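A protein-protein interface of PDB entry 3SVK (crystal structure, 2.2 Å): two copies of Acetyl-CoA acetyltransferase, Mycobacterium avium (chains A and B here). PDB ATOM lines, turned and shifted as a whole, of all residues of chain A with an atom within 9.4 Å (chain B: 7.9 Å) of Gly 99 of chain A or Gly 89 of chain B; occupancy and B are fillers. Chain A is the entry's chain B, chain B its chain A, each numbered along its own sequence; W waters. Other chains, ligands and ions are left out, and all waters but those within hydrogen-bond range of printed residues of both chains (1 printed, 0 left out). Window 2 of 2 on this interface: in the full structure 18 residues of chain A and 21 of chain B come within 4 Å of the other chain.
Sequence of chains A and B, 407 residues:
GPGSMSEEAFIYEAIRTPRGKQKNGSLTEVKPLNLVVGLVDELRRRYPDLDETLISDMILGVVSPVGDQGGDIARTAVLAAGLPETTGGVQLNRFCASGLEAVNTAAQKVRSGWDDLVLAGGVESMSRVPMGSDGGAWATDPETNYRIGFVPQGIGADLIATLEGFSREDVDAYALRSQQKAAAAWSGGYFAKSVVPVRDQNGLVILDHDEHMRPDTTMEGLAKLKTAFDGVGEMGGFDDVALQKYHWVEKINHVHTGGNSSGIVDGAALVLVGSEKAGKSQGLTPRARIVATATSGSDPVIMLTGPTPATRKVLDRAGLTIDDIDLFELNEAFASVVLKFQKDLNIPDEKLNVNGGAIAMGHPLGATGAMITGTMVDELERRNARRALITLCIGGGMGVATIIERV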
ATOM      1  N   GLN A  91      23.217 -28.900  10.952  1.00  0.00           N
ATOM      2  CA  GLN A  91      23.124 -30.157  11.685  1.00  0.00           C
ATOM      3  C   GLN A  91      24.025 -30.183  12.923  1.00  0.00           C
ATOM      4  O   GLN A  91      25.230 -29.902  12.842  1.00  0.00           O
ATOM      5  CB  GLN A  91      23.450 -31.354  10.782  1.00  0.00           C
ATOM      6  CG  GLN A  91      23.044 -32.667  11.426  1.00  0.00           C
ATOM      7  CD  GLN A  91      23.195 -33.862  10.488  1.00  0.00           C
ATOM      8  OE1 GLN A  91      22.306 -34.153   9.690  1.00  0.00           O
ATOM      9  NE2 GLN A  91      24.326 -34.563  10.592  1.00  0.00           N
ATOM     10  N   LEU A  92      23.419 -30.523  14.057  1.00  0.00           N
ATOM     11  CA  LEU A  92      24.065 -30.440  15.365  1.00  0.00           C
ATOM     12  C   LEU A  92      24.088 -31.806  16.070  1.00  0.00           C
ATOM     13  O   LEU A  92      23.051 -32.439  16.209  1.00  0.00           O
ATOM     14  CB  LEU A  92      23.330 -29.424  16.248  1.00  0.00           C
ATOM     15  CG  LEU A  92      23.301 -27.943  15.866  1.00  0.00           C
ATOM     16  CD1 LEU A  92      22.543 -27.170  16.927  1.00  0.00           C
ATOM     17  CD2 LEU A  92      24.721 -27.376  15.727  1.00  0.00           C
ATOM     18  N   ASN A  93      25.266 -32.262  16.505  1.00  0.00           N
ATOM     19  CA  ASN A  93      25.381 -33.425  17.422  1.00  0.00           C
ATOM     20  C   ASN A  93      25.797 -32.975  18.838  1.00  0.00           C
ATOM     21  O   ASN A  93      26.989 -32.868  19.162  1.00  0.00           O
ATOM     22  CB  ASN A  93      26.356 -34.483  16.911  1.00  0.00           C
ATOM     23  CG  ASN A  93      26.323 -35.772  17.765  1.00  0.00           C
ATOM     24  OD1 ASN A  93      25.574 -35.874  18.758  1.00  0.00           O
ATOM     25  ND2 ASN A  93      27.120 -36.763  17.369  1.00  0.00           N
ATOM     26  N   SER A  98      28.914 -29.690  18.102  1.00  0.00           N
ATOM     27  CA  SER A  98      29.552 -29.925  19.399  1.00  0.00           C
ATOM     28  C   SER A  98      29.632 -28.616  20.188  1.00  0.00           C
ATOM     29  O   SER A  98      30.314 -27.703  19.755  1.00  0.00           O
ATOM     30  CB  SER A  98      30.955 -30.511  19.210  1.00  0.00           C
ATOM     31  N   GLY A  99      28.943 -28.550  21.336  1.00  0.00           N
ATOM     32  CA  GLY A  99      28.881 -27.337  22.188  1.00  0.00           C
ATOM     33  C   GLY A  99      27.676 -26.432  21.898  1.00  0.00           C
ATOM     34  O   GLY A  99      27.479 -25.389  22.556  1.00  0.00           O
ATOM     35  N   LEU A 100      26.850 -26.817  20.930  1.00  0.00           N
ATOM     36  CA  LEU A 100      25.715 -26.015  20.581  1.00  0.00           C
ATOM     37  C   LEU A 100      24.441 -26.805  20.843  1.00  0.00           C
ATOM     38  O   LEU A 100      24.489 -28.012  21.166  1.00  0.00           O
ATOM     39  CB  LEU A 100      25.808 -25.596  19.119  1.00  0.00           C
ATOM     40  CG  LEU A 100      27.092 -24.837  18.738  1.00  0.00           C
ATOM     41  CD1 LEU A 100      27.189 -24.611  17.224  1.00  0.00           C
ATOM     42  CD2 LEU A 100      27.192 -23.503  19.492  1.00  0.00           C
ATOM     43  N   GLU A 101      23.313 -26.124  20.713  1.00  0.00           N
ATOM     44  CA  GLU A 101      22.033 -26.755  20.779  1.00  0.00           C
ATOM     45  C   GLU A 101      21.071 -25.999  19.875  1.00  0.00           C
ATOM     46  O   GLU A 101      21.226 -24.787  19.704  1.00  0.00           O
ATOM     47  CB  GLU A 101      21.553 -26.767  22.229  1.00  0.00           C
ATOM     48  CG  GLU A 101      20.224 -27.461  22.391  1.00  0.00           C
ATOM     49  CD  GLU A 101      19.046 -26.530  22.401  1.00  0.00           C
ATOM     50  OE1 GLU A 101      19.187 -25.444  22.950  1.00  0.00           O
ATOM     51  OE2 GLU A 101      17.958 -26.897  21.886  1.00  0.00           O
ATOM     52  N   ALA A 102      20.081 -26.708  19.320  1.00  0.00           N
ATOM     53  CA  ALA A 102      19.262 -26.178  18.234  1.00  0.00           C
ATOM     54  C   ALA A 102      18.508 -24.904  18.617  1.00  0.00           C
ATOM     55  O   ALA A 102      18.509 -23.924  17.910  1.00  0.00           O
ATOM     56  CB  ALA A 102      18.281 -27.251  17.709  1.00  0.00           C
ATOM     57  N   ASN A 104      18.798 -22.892  21.318  1.00  0.00           N
ATOM     58  CA  ASN A 104      19.791 -21.905  21.727  1.00  0.00           C
ATOM     59  C   ASN A 104      20.439 -21.259  20.482  1.00  0.00           C
ATOM     60  O   ASN A 104      20.606 -20.034  20.414  1.00  0.00           O
ATOM     61  CB  ASN A 104      20.823 -22.633  22.622  1.00  0.00           C
ATOM     62  CG  ASN A 104      22.083 -21.814  22.902  1.00  0.00           C
ATOM     63  OD1 ASN A 104      22.278 -21.302  23.997  1.00  0.00           O
ATOM     64  ND2 ASN A 104      22.958 -21.731  21.916  1.00  0.00           N
ATOM     65  N   THR A 105      20.785 -22.070  19.481  1.00  0.00           N
ATOM     66  CA  THR A 105      21.375 -21.506  18.264  1.00  0.00           C
ATOM     67  C   THR A 105      20.402 -20.627  17.499  1.00  0.00           C
ATOM     68  O   THR A 105      20.808 -19.591  16.976  1.00  0.00           O
ATOM     69  CB  THR A 105      21.948 -22.582  17.323  1.00  0.00           C
ATOM     70  OG1 THR A 105      22.990 -23.276  18.015  1.00  0.00           O
ATOM     71  CG2 THR A 105      22.541 -21.953  16.041  1.00  0.00           C
ATOM     72  N   GLN A 108      19.942 -17.184  19.148  1.00  0.00           N
ATOM     73  CA  GLN A 108      21.108 -16.296  18.947  1.00  0.00           C
ATOM     74  C   GLN A 108      21.152 -15.715  17.519  1.00  0.00           C
ATOM     75  O   GLN A 108      21.372 -14.514  17.362  1.00  0.00           O
ATOM     76  CB  GLN A 108      22.430 -16.986  19.367  1.00  0.00           C
ATOM     77  CG  GLN A 108      22.557 -16.990  20.909  1.00  0.00           C
ATOM     78  CD  GLN A 108      23.917 -17.421  21.416  1.00  0.00           C
ATOM     79  OE1 GLN A 108      24.332 -18.555  21.217  1.00  0.00           O
ATOM     80  NE2 GLN A 108      24.602 -16.520  22.095  1.00  0.00           N
ATOM     81  N   ALA A 294      21.869 -20.028  27.745  1.00  0.00           N
ATOM     82  CA  ALA A 294      23.244 -20.155  28.180  1.00  0.00           C
ATOM     83  C   ALA A 294      23.652 -21.609  28.162  1.00  0.00           C
ATOM     84  O   ALA A 294      22.808 -22.528  28.207  1.00  0.00           O
ATOM     85  CB  ALA A 294      23.442 -19.564  29.572  1.00  0.00           C
ATOM     86  N   THR A 295      24.962 -21.794  28.091  1.00  0.00           N
ATOM     87  CA  THR A 295      25.598 -23.082  27.956  1.00  0.00           C
ATOM     88  C   THR A 295      26.677 -23.216  29.016  1.00  0.00           C
ATOM     89  O   THR A 295      27.315 -22.238  29.387  1.00  0.00           O
ATOM     90  CB  THR A 295      26.236 -23.213  26.562  1.00  0.00           C
ATOM     91  OG1 THR A 295      25.224 -23.530  25.596  1.00  0.00           O
ATOM     92  CG2 THR A 295      27.267 -24.299  26.548  1.00  0.00           C
ATOM     93  N   SER A 296      26.890 -24.432  29.497  1.00  0.00           N
ATOM     94  CA  SER A 296      28.001 -24.690  30.386  1.00  0.00           C
ATOM     95  C   SER A 296      28.446 -26.144  30.314  1.00  0.00           C
ATOM     96  O   SER A 296      27.757 -27.039  30.805  1.00  0.00           O
ATOM     97  CB  SER A 296      27.647 -24.287  31.822  1.00  0.00           C
ATOM     98  OG  SER A 296      28.793 -24.432  32.648  1.00  0.00           O
ATOM     99  N   LYS A 313      23.623 -20.073  35.385  1.00  0.00           N
ATOM    100  CA  LYS A 313      24.143 -19.046  34.484  1.00  0.00           C
ATOM    101  C   LYS A 313      23.014 -18.354  33.722  1.00  0.00           C
ATOM    102  O   LYS A 313      22.998 -17.130  33.609  1.00  0.00           O
ATOM    103  CB  LYS A 313      25.105 -19.689  33.506  1.00  0.00           C
ATOM    104  CG  LYS A 313      25.947 -18.753  32.672  1.00  0.00           C
ATOM    105  CD  LYS A 313      27.110 -19.559  32.118  1.00  0.00           C
ATOM    106  CE  LYS A 313      27.661 -19.061  30.786  1.00  0.00           C
ATOM    107  NZ  LYS A 313      28.606 -20.113  30.269  1.00  0.00           N
ATOM    108  N   CYS A 393      21.218 -31.930  28.718  1.00  0.00           N
ATOM    109  CA  CYS A 393      22.607 -32.184  28.319  1.00  0.00           C
ATOM    110  C   CYS A 393      22.848 -32.040  26.790  1.00  0.00           C
ATOM    111  O   CYS A 393      22.038 -32.464  25.977  1.00  0.00           O
ATOM    112  CB  CYS A 393      23.044 -33.568  28.840  1.00  0.00           C
ATOM    113  SG  CYS A 393      23.008 -33.705  30.692  1.00  0.00           S
ATOM    114  N   ILE A 394      23.954 -31.400  26.403  1.00  0.00           N
ATOM    115  CA  ILE A 394      24.240 -31.101  24.969  1.00  0.00           C
ATOM    116  C   ILE A 394      24.911 -32.220  24.114  1.00  0.00           C
ATOM    117  O   ILE A 394      24.552 -32.385  22.920  1.00  0.00           O
ATOM    118  CB  ILE A 394      25.065 -29.807  24.842  1.00  0.00           C
ATOM    119  N   GLY A 395      25.859 -32.980  24.681  1.00  0.00           N
ATOM    120  CA  GLY A 395      26.260 -32.807  26.082  1.00  0.00           C
ATOM    121  C   GLY A 395      27.451 -33.571  26.615  1.00  0.00           C
ATOM    122  O   GLY A 395      27.385 -34.107  27.741  1.00  0.00           O
ATOM    123  N   GLY A 396      28.557 -33.573  25.870  1.00  0.00           N
ATOM    124  CA  GLY A 396      29.819 -34.161  26.360  1.00  0.00           C
ATOM    125  C   GLY A 396      30.325 -33.658  27.712  1.00  0.00           C
ATOM    126  O   GLY A 396      31.514 -33.375  27.880  1.00  0.00           O
ATOM    127  N   GLY A 397      29.434 -33.612  28.702  1.00  0.00           N
ATOM    128  CA  GLY A 397      29.691 -32.961  30.004  1.00  0.00           C
ATOM    129  C   GLY A 397      28.999 -31.607  30.116  1.00  0.00           C
ATOM    130  O   GLY A 397      29.010 -30.973  31.184  1.00  0.00           O
ATOM    131  N   MET A 398      28.369 -31.187  29.013  1.00  0.00           N
ATOM    132  CA  MET A 398      27.916 -29.802  28.826  1.00  0.00           C
ATOM    133  C   MET A 398      26.397 -29.677  28.824  1.00  0.00           C
ATOM    134  O   MET A 398      25.696 -30.476  28.210  1.00  0.00           O
ATOM    135  CB  MET A 398      28.459 -29.240  27.513  1.00  0.00           C
ATOM    136  CG  MET A 398      29.867 -28.625  27.641  1.00  0.00           C
ATOM    137  SD  MET A 398      30.512 -28.123  26.028  1.00  0.00           S
ATOM    138  CE  MET A 398      29.551 -26.638  25.746  1.00  0.00           C
ATOM    139  N   GLY A 399      25.912 -28.640  29.484  1.00  0.00           N
ATOM    140  CA  GLY A 399      24.499 -28.391  29.587  1.00  0.00           C
ATOM    141  C   GLY A 399      24.086 -27.087  28.958  1.00  0.00           C
ATOM    142  O   GLY A 399      24.898 -26.195  28.758  1.00  0.00           O
ATOM    143  N   VAL A 400      22.798 -26.993  28.703  1.00  0.00           N
ATOM    144  CA  VAL A 400      22.164 -25.837  28.124  1.00  0.00           C
ATOM    145  C   VAL A 400      20.890 -25.588  28.926  1.00  0.00           C
ATOM    146  O   VAL A 400      20.216 -26.531  29.320  1.00  0.00           O
ATOM    147  CB  VAL A 400      21.796 -26.099  26.662  1.00  0.00           C
ATOM    148  CG1 VAL A 400      21.365 -24.812  25.954  1.00  0.00           C
ATOM    149  CG2 VAL A 400      22.994 -26.710  25.932  1.00  0.00           C
ATOM    150  N   SER B  56      33.636 -16.404  26.785  1.00  0.00           N
ATOM    151  CA  SER B  56      32.603 -17.401  27.002  1.00  0.00           C
ATOM    152  C   SER B  56      32.824 -18.689  26.223  1.00  0.00           C
ATOM    153  O   SER B  56      32.407 -19.764  26.669  1.00  0.00           O
ATOM    154  CB  SER B  56      31.284 -16.823  26.553  1.00  0.00           C
ATOM    155  OG  SER B  56      31.281 -16.530  25.174  1.00  0.00           O
ATOM    156  N   ASP B  57      33.428 -18.591  25.037  1.00  0.00           N
ATOM    157  CA  ASP B  57      33.702 -19.788  24.222  1.00  0.00           C
ATOM    158  C   ASP B  57      34.950 -19.689  23.360  1.00  0.00           C
ATOM    159  O   ASP B  57      35.371 -18.591  22.967  1.00  0.00           O
ATOM    160  CB  ASP B  57      32.555 -20.084  23.270  1.00  0.00           C
ATOM    161  CG  ASP B  57      31.235 -20.204  23.973  1.00  0.00           C
ATOM    162  OD1 ASP B  57      30.560 -19.158  24.139  1.00  0.00           O
ATOM    163  OD2 ASP B  57      30.899 -21.351  24.351  1.00  0.00           O
ATOM    164  N   MET B  58      35.518 -20.856  23.070  1.00  0.00           N
ATOM    165  CA  MET B  58      36.483 -20.975  22.007  1.00  0.00           C
ATOM    166  C   MET B  58      35.844 -21.842  20.962  1.00  0.00           C
ATOM    167  O   MET B  58      35.408 -22.964  21.248  1.00  0.00           O
ATOM    168  CB  MET B  58      37.788 -21.636  22.463  1.00  0.00           C
ATOM    169  CG  MET B  58      38.677 -22.015  21.267  1.00  0.00           C
ATOM    170  SD  MET B  58      40.361 -21.528  21.507  1.00  0.00           S
ATOM    171  CE  MET B  58      40.844 -22.672  22.783  1.00  0.00           C
ATOM    172  N   ILE B  59      35.828 -21.319  19.747  1.00  0.00           N
ATOM    173  CA  ILE B  59      35.141 -21.949  18.641  1.00  0.00           C
ATOM    174  C   ILE B  59      36.212 -22.277  17.629  1.00  0.00           C
ATOM    175  O   ILE B  59      36.916 -21.375  17.172  1.00  0.00           O
ATOM    176  CB  ILE B  59      34.142 -20.983  18.015  1.00  0.00           C
ATOM    177  CG1 ILE B  59      33.074 -20.566  19.042  1.00  0.00           C
ATOM    178  CG2 ILE B  59      33.517 -21.616  16.768  1.00  0.00           C
ATOM    179  CD1 ILE B  59      32.196 -19.434  18.581  1.00  0.00           C
ATOM    180  N   LEU B  60      36.359 -23.570  17.312  1.00  0.00           N
ATOM    181  CA  LEU B  60      37.382 -24.031  16.394  1.00  0.00           C
ATOM    182  C   LEU B  60      36.792 -24.897  15.289  1.00  0.00           C
ATOM    183  O   LEU B  60      36.108 -25.873  15.560  1.00  0.00           O
ATOM    184  CB  LEU B  60      38.390 -24.867  17.157  1.00  0.00           C
ATOM    185  CG  LEU B  60      39.244 -24.198  18.215  1.00  0.00           C
ATOM    186  CD1 LEU B  60      40.174 -25.211  18.843  1.00  0.00           C
ATOM    187  CD2 LEU B  60      40.016 -23.081  17.619  1.00  0.00           C
ATOM    188  N   ASP B  72      37.474 -33.990  20.441  1.00  0.00           N
ATOM    189  CA  ASP B  72      36.922 -32.970  21.341  1.00  0.00           C
ATOM    190  C   ASP B  72      37.912 -31.803  21.507  1.00  0.00           C
ATOM    191  O   ASP B  72      38.192 -31.367  22.628  1.00  0.00           O
ATOM    192  CB  ASP B  72      36.573 -33.586  22.703  1.00  0.00           C
ATOM    193  N   ILE B  73      38.389 -31.283  20.383  1.00  0.00           N
ATOM    194  CA  ILE B  73      39.548 -30.371  20.334  1.00  0.00           C
ATOM    195  C   ILE B  73      39.330 -28.942  20.870  1.00  0.00           C
ATOM    196  O   ILE B  73      40.267 -28.302  21.365  1.00  0.00           O
ATOM    197  CB  ILE B  73      40.096 -30.259  18.887  1.00  0.00           C
ATOM    198  N   ALA B  74      38.127 -28.412  20.734  1.00  0.00           N
ATOM    199  CA  ALA B  74      37.835 -27.083  21.284  1.00  0.00           C
ATOM    200  C   ALA B  74      37.756 -27.167  22.816  1.00  0.00           C
ATOM    201  O   ALA B  74      38.261 -26.307  23.513  1.00  0.00           O
ATOM    202  CB  ALA B  74      36.529 -26.512  20.690  1.00  0.00           C
ATOM    203  N   ARG B  75      37.143 -28.223  23.328  1.00  0.00           N
ATOM    204  CA  ARG B  75      37.053 -28.404  24.774  1.00  0.00           C
ATOM    205  C   ARG B  75      38.455 -28.686  25.359  1.00  0.00           C
ATOM    206  O   ARG B  75      38.835 -28.120  26.378  1.00  0.00           O
ATOM    207  CB  ARG B  75      36.056 -29.516  25.124  1.00  0.00           C
ATOM    208  N   THR B  76      39.238 -29.530  24.698  1.00  0.00           N
ATOM    209  CA  THR B  76      40.591 -29.828  25.174  1.00  0.00           C
ATOM    210  C   THR B  76      41.507 -28.586  25.121  1.00  0.00           C
ATOM    211  O   THR B  76      42.325 -28.366  26.022  1.00  0.00           O
ATOM    212  CB  THR B  76      41.195 -30.995  24.390  1.00  0.00           C
ATOM    213  OG1 THR B  76      40.356 -32.138  24.564  1.00  0.00           O
ATOM    214  CG2 THR B  76      42.595 -31.318  24.875  1.00  0.00           C
ATOM    215  N   ALA B  77      41.301 -27.751  24.110  1.00  0.00           N
ATOM    216  CA  ALA B  77      42.079 -26.545  23.917  1.00  0.00           C
ATOM    217  C   ALA B  77      41.896 -25.568  25.051  1.00  0.00           C
ATOM    218  O   ALA B  77      42.854 -24.980  25.556  1.00  0.00           O
ATOM    219  CB  ALA B  77      41.691 -25.871  22.582  1.00  0.00           C
ATOM    220  N   VAL B  78      40.650 -25.365  25.418  1.00  0.00           N
ATOM    221  CA  VAL B  78      40.304 -24.495  26.521  1.00  0.00           C
ATOM    222  C   VAL B  78      41.041 -24.940  27.795  1.00  0.00           C
ATOM    223  O   VAL B  78      41.571 -24.105  28.532  1.00  0.00           O
ATOM    224  CB  VAL B  78      38.780 -24.543  26.762  1.00  0.00           C
ATOM    225  CG1 VAL B  78      38.437 -24.017  28.151  1.00  0.00           C
ATOM    226  CG2 VAL B  78      38.034 -23.793  25.636  1.00  0.00           C
ATOM    227  N   PRO B  84      39.516 -20.153  31.526  1.00  0.00           N
ATOM    228  CA  PRO B  84      38.631 -20.483  32.665  1.00  0.00           C
ATOM    229  C   PRO B  84      37.711 -21.691  32.437  1.00  0.00           C
ATOM    230  O   PRO B  84      37.426 -22.063  31.302  1.00  0.00           O
ATOM    231  CB  PRO B  84      37.811 -19.206  32.855  1.00  0.00           C
ATOM    232  CG  PRO B  84      38.701 -18.118  32.342  1.00  0.00           C
ATOM    233  CD  PRO B  84      39.449 -18.725  31.172  1.00  0.00           C
ATOM    234  N   GLU B  85      37.249 -22.290  33.527  1.00  0.00           N
ATOM    235  CA  GLU B  85      36.316 -23.419  33.457  1.00  0.00           C
ATOM    236  C   GLU B  85      34.945 -22.940  32.965  1.00  0.00           C
ATOM    237  O   GLU B  85      34.122 -23.751  32.531  1.00  0.00           O
ATOM    238  CB  GLU B  85      36.199 -24.107  34.830  1.00  0.00           C
ATOM    239  N   THR B  86      34.718 -21.622  33.047  1.00  0.00           N
ATOM    240  CA  THR B  86      33.524 -20.963  32.500  1.00  0.00           C
ATOM    241  C   THR B  86      33.544 -20.790  30.978  1.00  0.00           C
ATOM    242  O   THR B  86      32.511 -20.505  30.367  1.00  0.00           O
ATOM    243  CB  THR B  86      33.328 -19.556  33.107  1.00  0.00           C
ATOM    244  N   THR B  87      34.713 -20.902  30.363  1.00  0.00           N
ATOM    245  CA  THR B  87      34.807 -20.817  28.910  1.00  0.00           C
ATOM    246  C   THR B  87      34.441 -22.200  28.366  1.00  0.00           C
ATOM    247  O   THR B  87      35.029 -23.189  28.798  1.00  0.00           O
ATOM    248  CB  THR B  87      36.237 -20.409  28.467  1.00  0.00           C
ATOM    249  OG1 THR B  87      36.699 -19.288  29.247  1.00  0.00           O
ATOM    250  CG2 THR B  87      36.272 -20.008  26.979  1.00  0.00           C
ATOM    251  N   GLY B  88      33.452 -22.282  27.473  1.00  0.00           N
ATOM    252  CA  GLY B  88      33.108 -23.531  26.782  1.00  0.00           C
ATOM    253  C   GLY B  88      33.843 -23.702  25.448  1.00  0.00           C
ATOM    254  O   GLY B  88      34.422 -22.765  24.913  1.00  0.00           O
ATOM    255  N   GLY B  89      33.830 -24.915  24.911  1.00  0.00           N
ATOM    256  CA  GLY B  89      34.388 -25.187  23.601  1.00  0.00           C
ATOM    257  C   GLY B  89      33.326 -25.560  22.583  1.00  0.00           C
ATOM    258  O   GLY B  89      32.404 -26.320  22.896  1.00  0.00           O
ATOM    259  N   VAL B  90      33.447 -25.024  21.372  1.00  0.00           N
ATOM    260  CA  VAL B  90      32.526 -25.305  20.284  1.00  0.00           C
ATOM    261  C   VAL B  90      33.353 -25.774  19.099  1.00  0.00           C
ATOM    262  O   VAL B  90      34.255 -25.066  18.647  1.00  0.00           O
ATOM    263  CB  VAL B  90      31.732 -24.035  19.888  1.00  0.00           C
ATOM    264  CG1 VAL B  90      30.856 -24.272  18.632  1.00  0.00           C
ATOM    265  CG2 VAL B  90      30.883 -23.560  21.043  1.00  0.00           C
ATOM    266  N   GLN B  91      33.058 -26.977  18.610  1.00  0.00           N
ATOM    267  CA  GLN B  91      33.805 -27.579  17.513  1.00  0.00           C
ATOM    268  C   GLN B  91      32.986 -27.627  16.231  1.00  0.00           C
ATOM    269  O   GLN B  91      31.902 -28.170  16.220  1.00  0.00           O
ATOM    270  CB  GLN B  91      34.216 -28.990  17.883  1.00  0.00           C
ATOM    271  CG  GLN B  91      35.171 -29.555  16.874  1.00  0.00           C
ATOM    272  CD  GLN B  91      35.897 -30.771  17.384  1.00  0.00           C
ATOM    273  OE1 GLN B  91      37.112 -30.735  17.538  1.00  0.00           O
ATOM    274  NE2 GLN B  91      35.167 -31.850  17.634  1.00  0.00           N
ATOM    275  N   LEU B  92      33.501 -27.035  15.157  1.00  0.00           N
ATOM    276  CA  LEU B  92      32.781 -26.997  13.889  1.00  0.00           C
ATOM    277  C   LEU B  92      33.514 -27.874  12.871  1.00  0.00           C
ATOM    278  O   LEU B  92      34.579 -27.509  12.372  1.00  0.00           O
ATOM    279  CB  LEU B  92      32.655 -25.556  13.394  1.00  0.00           C
ATOM    280  CG  LEU B  92      31.898 -24.594  14.296  1.00  0.00           C
ATOM    281  CD1 LEU B  92      31.938 -23.207  13.706  1.00  0.00           C
ATOM    282  CD2 LEU B  92      30.431 -25.052  14.576  1.00  0.00           C
ATOM    283  N   ALA B  97      28.764 -30.269  14.213  1.00  0.00           N
ATOM    284  CA  ALA B  97      28.115 -29.005  13.857  1.00  0.00           C
ATOM    285  C   ALA B  97      28.467 -28.500  12.431  1.00  0.00           C
ATOM    286  O   ALA B  97      29.530 -27.891  12.211  1.00  0.00           O
ATOM    287  CB  ALA B  97      28.400 -27.958  14.895  1.00  0.00           C
ATOM    288  N   LYS B 109      26.850 -14.601  18.271  1.00  0.00           N
ATOM    289  CA  LYS B 109      26.826 -14.710  19.718  1.00  0.00           C
ATOM    290  C   LYS B 109      27.014 -13.349  20.374  1.00  0.00           C
ATOM    291  O   LYS B 109      26.317 -13.015  21.305  1.00  0.00           O
ATOM    292  CB  LYS B 109      27.887 -15.662  20.240  1.00  0.00           C
ATOM    293  CG  LYS B 109      27.655 -17.164  20.004  1.00  0.00           C
ATOM    294  CD  LYS B 109      28.796 -18.013  20.613  1.00  0.00           C
ATOM    295  CE  LYS B 109      28.361 -19.434  20.959  1.00  0.00           C
ATOM    296  NZ  LYS B 109      27.241 -19.439  21.985  1.00  0.00           N
HETATM  297  O   HOH W   1      29.524 -23.856  24.748  1.00  0.00           O
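Of the 23 printed residues of chain A, 7 touch a printed residue of chain B.
Printed residues of chain A that touch a printed residue of chain B: Gln 91, Leu 92, Ser 98, Gly 99, Leu 100, Gln 108 and Lys 313.
Of the 23 printed residues of chain B, 6 touch a printed residue of chain A.
Hydrophobic or aromatic side chains of chain B that line the printed part of chain A: Val 90 and Ala 97.
Among the printed residues, pairs that only touch across the chains: Gln 91 of chain A with Ala 97 of chain B (3.2 Å), Ser 98 of chain A with Val 90 of chain B (3.3 Å), Ser 98 of chain A with Ala 97 of chain B (3.7 Å), Gly 99 of chain A with Gly 89 of chain B (3.7 Å), Leu 100 of chain A with Val 90 of chain B (3.8 Å), Leu 92 of chain A with Ala 97 of chain B (3.8 Å) and Lys 313 of chain A with Thr 86 of chain B (3.9 Å).
OD1 of Asp 57 of chain B is in salt-bridge range of NZ of Lys 109 of chain B, 3.97 Å away.
O of Met 58 of chain B is in hydrogen-bond range of N of Val 90 of chain B (2.8 Å).
The backbone NH (N) of Leu 60 of chain B lies within hydrogen-bond range of the backbone carbonyl oxygen (O) of Val 90 of chain B.
OE1 of Gln 91 of chain B is in hydrogen-bond range of N of Ile 73 of chain B (3.2 Å).
NZ of Lys 313 of chain A is in hydrogen-bond range of O of Thr 295 of chain A, 2.6 Å away.
The backbone NH (N) of Gln 91 of chain B sits at hydrogen-bond distance from the backbone carbonyl oxygen (O) of Ser 98 of chain A (3.1 Å).
The side-chain amide oxygen (OE1) of Gln 108 of chain A lies within hydrogen-bond range of the side-chain amino group (NZ) of Lys 109 of chain B, 3.1 Å away.
Printed residues of chain B within 4 Å of Gly 99 of chain A: Gly 89 (3.7 Å).
Of the printed residues of chain A, Gly 89 of chain B touches Gly 99 (3.7 Å).
No residue of chain A comes within 4 Å of Gly 88 of chain B.
Of chain A, only Ser 98 and Leu 100 come within 4 Å of Val 90 of chain B.
Printed residues of chain A within 4 Å of Ala 97 of chain B: Gln 91, Leu 92 and Ser 98.
Printed residues of chain A within 4 Å of Thr 86 of chain B: Lys 313.
Printed residues of chain A within 4 Å of Gln 91 of chain B: Ser 98 (3.1 Å).
Printed residues of chain B within 4 Å of Ser 98 of chain A: Val 90, Gln 91 and Ala 97.
The nearest residue of chain B that does not touch Gly 99 of chain A is Val 90 of chain B (4.1 Å).
Water W1 lies within hydrogen-bond range of the side-chain carboxylate of Asp 57 of chain B (2.9 Å) and the backbone carbonyl oxygen of Gly 99 of chain A (3.4 Å).
Positions printed for both chains: 91 and 92.
Of the 9 pairs that touch across the chains among the printed residues, none has its exchanged pair printed and touching as well.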
